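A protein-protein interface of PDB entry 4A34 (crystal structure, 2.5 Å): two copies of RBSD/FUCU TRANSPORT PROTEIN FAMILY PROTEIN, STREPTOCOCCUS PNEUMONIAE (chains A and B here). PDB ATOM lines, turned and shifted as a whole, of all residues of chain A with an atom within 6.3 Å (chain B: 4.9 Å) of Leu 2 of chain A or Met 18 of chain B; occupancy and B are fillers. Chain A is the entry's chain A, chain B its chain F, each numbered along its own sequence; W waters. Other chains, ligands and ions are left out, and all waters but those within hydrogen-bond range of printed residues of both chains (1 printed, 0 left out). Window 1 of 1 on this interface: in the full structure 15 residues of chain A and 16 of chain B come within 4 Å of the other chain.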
ATOM      1  N   LEU A   2     -24.804  18.958  21.622  1.00  0.00           N
ATOM      2  CA  LEU A   2     -25.251  17.817  22.469  1.00  0.00           C
ATOM      3  C   LEU A   2     -24.515  16.524  22.131  1.00  0.00           C
ATOM      4  O   LEU A   2     -23.993  16.370  21.023  1.00  0.00           O
ATOM      5  CB  LEU A   2     -26.758  17.595  22.321  1.00  0.00           C
ATOM      6  CG  LEU A   2     -27.756  18.704  22.669  1.00  0.00           C
ATOM      7  CD1 LEU A   2     -29.153  18.218  22.350  1.00  0.00           C
ATOM      8  CD2 LEU A   2     -27.656  19.142  24.127  1.00  0.00           C
ATOM      9  N   LYS A   3     -24.493  15.595  23.089  1.00  0.00           N
ATOM     10  CA  LYS A   3     -23.864  14.285  22.924  1.00  0.00           C
ATOM     11  C   LYS A   3     -24.562  13.453  21.859  1.00  0.00           C
ATOM     12  O   LYS A   3     -25.775  13.557  21.684  1.00  0.00           O
ATOM     13  CB  LYS A   3     -23.897  13.530  24.251  1.00  0.00           C
ATOM     14  CG  LYS A   3     -22.704  13.797  25.171  1.00  0.00           C
ATOM     15  CD  LYS A   3     -23.123  13.967  26.636  1.00  0.00           C
ATOM     16  CE  LYS A   3     -24.023  12.840  27.139  1.00  0.00           C
ATOM     17  NZ  LYS A   3     -24.845  13.267  28.309  1.00  0.00           N
ATOM     18  N   HIS A   4     -23.790  12.627  21.157  1.00  0.00           N
ATOM     19  CA  HIS A   4     -24.320  11.630  20.208  1.00  0.00           C
ATOM     20  C   HIS A   4     -25.063  12.215  18.998  1.00  0.00           C
ATOM     21  O   HIS A   4     -25.722  11.482  18.256  1.00  0.00           O
ATOM     22  CB  HIS A   4     -25.196  10.579  20.920  1.00  0.00           C
ATOM     23  CG  HIS A   4     -24.604  10.050  22.192  1.00  0.00           C
ATOM     24  ND1 HIS A   4     -25.251  10.136  23.407  1.00  0.00           N
ATOM     25  CD2 HIS A   4     -23.418   9.440  22.440  1.00  0.00           C
ATOM     26  CE1 HIS A   4     -24.494   9.600  24.348  1.00  0.00           C
ATOM     27  NE2 HIS A   4     -23.377   9.170  23.788  1.00  0.00           N
ATOM     28  N   ILE A   5     -24.959  13.528  18.814  1.00  0.00           N
ATOM     29  CA  ILE A   5     -25.407  14.190  17.593  1.00  0.00           C
ATOM     30  C   ILE A   5     -24.160  14.737  16.900  1.00  0.00           C
ATOM     31  O   ILE A   5     -23.310  15.327  17.567  1.00  0.00           O
ATOM     32  CB  ILE A   5     -26.390  15.351  17.903  1.00  0.00           C
ATOM     33  CG1 ILE A   5     -27.705  14.806  18.469  1.00  0.00           C
ATOM     34  CG2 ILE A   5     -26.672  16.193  16.657  1.00  0.00           C
ATOM     35  CD1 ILE A   5     -28.413  15.779  19.373  1.00  0.00           C
ATOM     36  N   PRO A   6     -24.028  14.526  15.574  1.00  0.00           N
ATOM     37  CA  PRO A   6     -22.927  15.136  14.826  1.00  0.00           C
ATOM     38  C   PRO A   6     -22.792  16.638  15.096  1.00  0.00           C
ATOM     39  O   PRO A   6     -23.800  17.344  15.249  1.00  0.00           O
ATOM     40  CB  PRO A   6     -23.323  14.893  13.370  1.00  0.00           C
ATOM     41  CG  PRO A   6     -24.091  13.642  13.399  1.00  0.00           C
ATOM     42  CD  PRO A   6     -24.828  13.624  14.722  1.00  0.00           C
ATOM     43  N   LYS A   7     -21.549  17.113  15.155  1.00  0.00           N
ATOM     44  CA  LYS A   7     -21.264  18.503  15.547  1.00  0.00           C
ATOM     45  C   LYS A   7     -21.381  19.548  14.410  1.00  0.00           C
ATOM     46  O   LYS A   7     -21.283  20.751  14.666  1.00  0.00           O
ATOM     47  CB  LYS A   7     -19.898  18.606  16.260  1.00  0.00           C
ATOM     48  CG  LYS A   7     -19.826  17.877  17.619  1.00  0.00           C
ATOM     49  CD  LYS A   7     -19.274  18.770  18.738  1.00  0.00           C
ATOM     50  CE  LYS A   7     -20.355  19.729  19.294  1.00  0.00           C
ATOM     51  NZ  LYS A   7     -19.832  20.836  20.175  1.00  0.00           N
ATOM     52  N   ILE A   9     -24.090  19.629  12.022  1.00  0.00           N
ATOM     53  CA  ILE A   9     -25.461  19.954  11.654  1.00  0.00           C
ATOM     54  C   ILE A   9     -26.087  20.874  12.711  1.00  0.00           C
ATOM     55  O   ILE A   9     -26.081  20.574  13.901  1.00  0.00           O
ATOM     56  CB  ILE A   9     -26.333  18.692  11.287  1.00  0.00           C
ATOM     57  CG1 ILE A   9     -27.794  18.859  11.725  1.00  0.00           C
ATOM     58  CG2 ILE A   9     -25.739  17.405  11.842  1.00  0.00           C
ATOM     59  CD1 ILE A   9     -28.092  18.312  13.094  1.00  0.00           C
ATOM     60  N   SER A  10     -26.600  22.006  12.239  1.00  0.00           N
ATOM     61  CA  SER A  10     -27.101  23.083  13.082  1.00  0.00           C
ATOM     62  C   SER A  10     -28.455  22.783  13.744  1.00  0.00           C
ATOM     63  O   SER A  10     -29.164  21.859  13.331  1.00  0.00           O
ATOM     64  CB  SER A  10     -27.190  24.372  12.258  1.00  0.00           C
ATOM     65  OG  SER A  10     -28.190  24.288  11.253  1.00  0.00           O
ATOM     66  N   PRO A  11     -28.811  23.567  14.786  1.00  0.00           N
ATOM     67  CA  PRO A  11     -30.092  23.461  15.473  1.00  0.00           C
ATOM     68  C   PRO A  11     -31.298  23.456  14.549  1.00  0.00           C
ATOM     69  O   PRO A  11     -32.138  22.559  14.649  1.00  0.00           O
ATOM     70  CB  PRO A  11     -30.099  24.695  16.368  1.00  0.00           C
ATOM     71  CG  PRO A  11     -28.689  24.861  16.730  1.00  0.00           C
ATOM     72  CD  PRO A  11     -27.902  24.480  15.507  1.00  0.00           C
ATOM     73  N   ASP A  12     -31.391  24.427  13.648  1.00  0.00           N
ATOM     74  CA  ASP A  12     -32.549  24.469  12.771  1.00  0.00           C
ATOM     75  C   ASP A  12     -32.455  23.393  11.701  1.00  0.00           C
ATOM     76  O   ASP A  12     -33.480  22.929  11.196  1.00  0.00           O
ATOM     77  CB  ASP A  12     -32.788  25.868  12.169  1.00  0.00           C
ATOM     78  CG  ASP A  12     -34.272  26.121  11.819  1.00  0.00           C
ATOM     79  OD1 ASP A  12     -35.147  25.261  12.094  1.00  0.00           O
ATOM     80  OD2 ASP A  12     -34.576  27.196  11.265  1.00  0.00           O
ATOM     81  N   LEU A  14     -31.359  20.284  12.260  1.00  0.00           N
ATOM     82  CA  LEU A  14     -31.873  19.064  12.872  1.00  0.00           C
ATOM     83  C   LEU A  14     -33.391  19.058  12.927  1.00  0.00           C
ATOM     84  O   LEU A  14     -34.023  18.108  12.474  1.00  0.00           O
ATOM     85  CB  LEU A  14     -31.284  18.840  14.255  1.00  0.00           C
ATOM     86  CG  LEU A  14     -31.265  17.410  14.803  1.00  0.00           C
ATOM     87  CD1 LEU A  14     -31.180  16.347  13.703  1.00  0.00           C
ATOM     88  CD2 LEU A  14     -30.105  17.262  15.759  1.00  0.00           C
ATOM     89  N   LEU B  14     -35.456  19.279  20.437  1.00  0.00           N
ATOM     90  CA  LEU B  14     -34.060  19.015  20.123  1.00  0.00           C
ATOM     91  C   LEU B  14     -33.344  20.302  19.730  1.00  0.00           C
ATOM     92  O   LEU B  14     -32.230  20.578  20.212  1.00  0.00           O
ATOM     93  CB  LEU B  14     -33.925  17.977  19.007  1.00  0.00           C
ATOM     94  CG  LEU B  14     -32.769  16.989  19.186  1.00  0.00           C
ATOM     95  CD1 LEU B  14     -32.767  15.977  18.073  1.00  0.00           C
ATOM     96  CD2 LEU B  14     -31.415  17.670  19.280  1.00  0.00           C
ATOM     97  N   LYS B  15     -33.989  21.075  18.852  1.00  0.00           N
ATOM     98  CA  LYS B  15     -33.504  22.398  18.486  1.00  0.00           C
ATOM     99  C   LYS B  15     -33.173  23.214  19.733  1.00  0.00           C
ATOM    100  O   LYS B  15     -32.024  23.652  19.910  1.00  0.00           O
ATOM    101  CB  LYS B  15     -34.517  23.139  17.615  1.00  0.00           C
ATOM    102  CG  LYS B  15     -34.063  24.526  17.210  1.00  0.00           C
ATOM    103  CD  LYS B  15     -35.058  25.193  16.306  1.00  0.00           C
ATOM    104  CE  LYS B  15     -34.586  26.585  15.905  1.00  0.00           C
ATOM    105  NZ  LYS B  15     -35.066  27.655  16.827  1.00  0.00           N
ATOM    106  N   THR B  16     -34.161  23.402  20.606  1.00  0.00           N
ATOM    107  CA  THR B  16     -33.939  24.246  21.781  1.00  0.00           C
ATOM    108  C   THR B  16     -32.823  23.667  22.662  1.00  0.00           C
ATOM    109  O   THR B  16     -31.962  24.410  23.123  1.00  0.00           O
ATOM    110  CB  THR B  16     -35.265  24.688  22.522  1.00  0.00           C
ATOM    111  OG1 THR B  16     -35.141  24.564  23.948  1.00  0.00           O
ATOM    112  CG2 THR B  16     -36.463  23.904  22.047  1.00  0.00           C
ATOM    113  N   LEU B  17     -32.791  22.343  22.809  1.00  0.00           N
ATOM    114  CA  LEU B  17     -31.683  21.675  23.512  1.00  0.00           C
ATOM    115  C   LEU B  17     -30.293  22.004  22.928  1.00  0.00           C
ATOM    116  O   LEU B  17     -29.333  22.217  23.674  1.00  0.00           O
ATOM    117  CB  LEU B  17     -31.903  20.156  23.597  1.00  0.00           C
ATOM    118  CG  LEU B  17     -33.094  19.594  24.386  1.00  0.00           C
ATOM    119  CD1 LEU B  17     -33.365  18.145  23.990  1.00  0.00           C
ATOM    120  CD2 LEU B  17     -32.933  19.710  25.891  1.00  0.00           C
ATOM    121  N   MET B  18     -30.192  22.069  21.604  1.00  0.00           N
ATOM    122  CA  MET B  18     -28.923  22.422  20.947  1.00  0.00           C
ATOM    123  C   MET B  18     -28.587  23.908  20.988  1.00  0.00           C
ATOM    124  O   MET B  18     -27.410  24.275  21.042  1.00  0.00           O
ATOM    125  CB  MET B  18     -28.930  21.962  19.502  1.00  0.00           C
ATOM    126  CG  MET B  18     -28.701  20.483  19.332  1.00  0.00           C
ATOM    127  SD  MET B  18     -29.180  20.058  17.665  1.00  0.00           S
ATOM    128  CE  MET B  18     -27.840  20.815  16.729  1.00  0.00           C
ATOM    129  N   GLU B  19     -29.626  24.749  20.936  1.00  0.00           N
ATOM    130  CA  GLU B  19     -29.483  26.196  21.055  1.00  0.00           C
ATOM    131  C   GLU B  19     -28.992  26.580  22.431  1.00  0.00           C
ATOM    132  O   GLU B  19     -28.345  27.615  22.605  1.00  0.00           O
ATOM    133  CB  GLU B  19     -30.825  26.886  20.877  1.00  0.00           C
ATOM    134  CG  GLU B  19     -31.493  26.686  19.559  1.00  0.00           C
ATOM    135  CD  GLU B  19     -32.757  27.477  19.483  1.00  0.00           C
ATOM    136  OE1 GLU B  19     -33.518  27.483  20.478  1.00  0.00           O
ATOM    137  OE2 GLU B  19     -32.990  28.106  18.437  1.00  0.00           O
ATOM    138  N   MET B  20     -29.340  25.763  23.418  1.00  0.00           N
ATOM    139  CA  MET B  20     -28.942  26.020  24.786  1.00  0.00           C
ATOM    140  C   MET B  20     -27.435  25.928  24.919  1.00  0.00           C
ATOM    141  O   MET B  20     -26.796  25.076  24.304  1.00  0.00           O
ATOM    142  CB  MET B  20     -29.630  25.057  25.739  1.00  0.00           C
ATOM    143  CG  MET B  20     -31.025  25.482  26.112  1.00  0.00           C
ATOM    144  SD  MET B  20     -31.763  24.365  27.312  1.00  0.00           S
ATOM    145  CE  MET B  20     -32.408  23.112  26.236  1.00  0.00           C
ATOM    146  N   LEU B  60     -28.755  12.974  26.046  1.00  0.00           N
ATOM    147  CA  LEU B  60     -28.242  13.929  25.062  1.00  0.00           C
ATOM    148  C   LEU B  60     -27.508  15.119  25.666  1.00  0.00           C
ATOM    149  O   LEU B  60     -26.605  15.666  25.042  1.00  0.00           O
ATOM    150  CB  LEU B  60     -29.379  14.457  24.182  1.00  0.00           C
ATOM    151  CG  LEU B  60     -30.195  13.514  23.300  1.00  0.00           C
ATOM    152  CD1 LEU B  60     -31.561  14.116  23.082  1.00  0.00           C
ATOM    153  CD2 LEU B  60     -29.515  13.268  21.976  1.00  0.00           C
ATOM    154  N   MET B  61     -27.899  15.530  26.867  1.00  0.00           N
ATOM    155  CA  MET B  61     -27.405  16.782  27.438  1.00  0.00           C
ATOM    156  C   MET B  61     -26.690  16.611  28.778  1.00  0.00           C
ATOM    157  O   MET B  61     -27.275  16.091  29.726  1.00  0.00           O
ATOM    158  CB  MET B  61     -28.548  17.791  27.592  1.00  0.00           C
ATOM    159  CG  MET B  61     -28.110  19.144  28.144  1.00  0.00           C
ATOM    160  SD  MET B  61     -29.491  20.242  28.459  1.00  0.00           S
ATOM    161  CE  MET B  61     -30.091  19.662  30.041  1.00  0.00           C
ATOM    162  N   LYS B 137     -27.806  23.085  31.819  1.00  0.00           N
ATOM    163  CA  LYS B 137     -26.903  22.516  30.812  1.00  0.00           C
ATOM    164  C   LYS B 137     -25.424  22.675  31.188  1.00  0.00           C
ATOM    165  O   LYS B 137     -25.020  23.696  31.746  1.00  0.00           O
ATOM    166  CB  LYS B 137     -27.191  23.111  29.427  1.00  0.00           C
ATOM    167  CG  LYS B 137     -26.346  22.524  28.302  1.00  0.00           C
ATOM    168  CD  LYS B 137     -26.953  22.785  26.942  1.00  0.00           C
ATOM    169  CE  LYS B 137     -26.165  22.107  25.844  1.00  0.00           C
ATOM    170  NZ  LYS B 137     -26.788  22.348  24.514  1.00  0.00           N
ATOM    171  N   VAL B 140     -20.047  20.589  26.665  1.00  0.00           N
ATOM    172  CA  VAL B 140     -19.973  19.448  25.758  1.00  0.00           C
ATOM    173  C   VAL B 140     -18.541  19.350  25.236  1.00  0.00           C
ATOM    174  O   VAL B 140     -18.053  20.263  24.550  1.00  0.00           O
ATOM    175  CB  VAL B 140     -20.986  19.568  24.576  1.00  0.00           C
ATOM    176  CG1 VAL B 140     -20.777  18.455  23.565  1.00  0.00           C
ATOM    177  CG2 VAL B 140     -22.418  19.546  25.086  1.00  0.00           C
HETATM  178  O   HOH W   1     -26.427  14.065  31.148  1.00  0.00           O
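Leu 2 of chain A touches six residues of chain B. Of the printed residues of chain B, Lys 3 of chain A touches Leu 60 (2.9 Å) and Met 61 (3.8 Å). His 4 of chain A touches none of the printed residues of chain B. Of the printed residues of chain B, Ile 5 of chain A touches Leu 14 and Leu 60. Pro 6 of chain A touches none of the printed residues of chain B. Printed residues of chain B within 4 Å of Ser 10 of chain A: Met 18 (3.6 Å). Of the printed residues of chain A, Leu 14 of chain B touches Leu 2 (3.9 Å), Ile 5 (3.5 Å) and Leu 14 (3.8 Å). Of the printed residues of chain A, Lys 15 of chain B touches Pro 11 (3.8 Å). The nearest residue of chain B that does not touch Leu 2 of chain A is Val 140 of chain B (4.2 Å). The nearest residue of chain A that does not touch Met 18 of chain B is Ile 5 of chain A (4.7 Å). The nearest printed residue of chain A that does not touch Lys 137 of chain B is Lys 3 of chain A (7.3 Å).
Water W1 bridges O of Met 61 of chain B (2.6 Å) and NZ of Lys 3 of chain A (3.3 Å).
Leu 14 of chain B touches its own counterpart, Leu 14 of chain A. Of the 16 pairs that touch across the chains among the printed residues, 1 has its exchanged pair printed and touching as well.
The side-chain amino group (NZ) of Lys 15 of chain B is in salt-bridge range of the side-chain carboxylate (OE2) of Glu 19 of chain B (2.7 Å). The backbone carbonyl oxygen (O) of Leu 17 of chain B lies within hydrogen-bond range of the side-chain amino group (NZ) of Lys 137 of chain B, at 2.7 Å. The backbone carbonyl oxygen of Met 20 of chain B sits at hydrogen-bond distance from the side-chain amino group of Lys 137 of chain B (2.7 Å).
N of Lys 3 of chain A is in hydrogen-bond range of O of Leu 60 of chain B, at 2.9 Å.
Of the 11 printed residues of chain A, 7 touch a printed residue of chain B. Printed residues of chain A that touch a printed residue of chain B: Leu 2, Lys 3, Ile 5, Ile 9, Ser 10, Pro 11 and Leu 14. Hydrophobic or aromatic side chains of chain A within 4 Å of the printed part of chain B: Leu 2, Ile 5, Pro 11 and Leu 14. Among the printed residues, no Asp or Glu carboxylate lies within 4 Å of a Lys or Arg side-chain nitrogen of the other chain.
Among the printed residues, merely in contact across the chains: Leu 2 of chain A with Leu 14 of chain B, Leu 2 of chain A with Leu 17 of chain B, Leu 2 of chain A with Met 18 of chain B, Leu 2 of chain A with Leu 60 of chain B, Leu 2 of chain A with Met 61 of chain B, Leu 2 of chain A with Lys 137 of chain B, Lys 3 of chain A with Met 61 of chain B, Ile 5 of chain A with Leu 14 of chain B, Ile 5 of chain A with Leu 60 of chain B, Ile 9 of chain A with Met 18 of chain B, Ser 10 of chain A with Met 18 of chain B, Pro 11 of chain A with Lys 15 of chain B, Pro 11 of chain A with Met 18 of chain B, Leu 14 of chain A with Leu 14 of chain B and Leu 14 of chain A with Met 18 of chain B.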
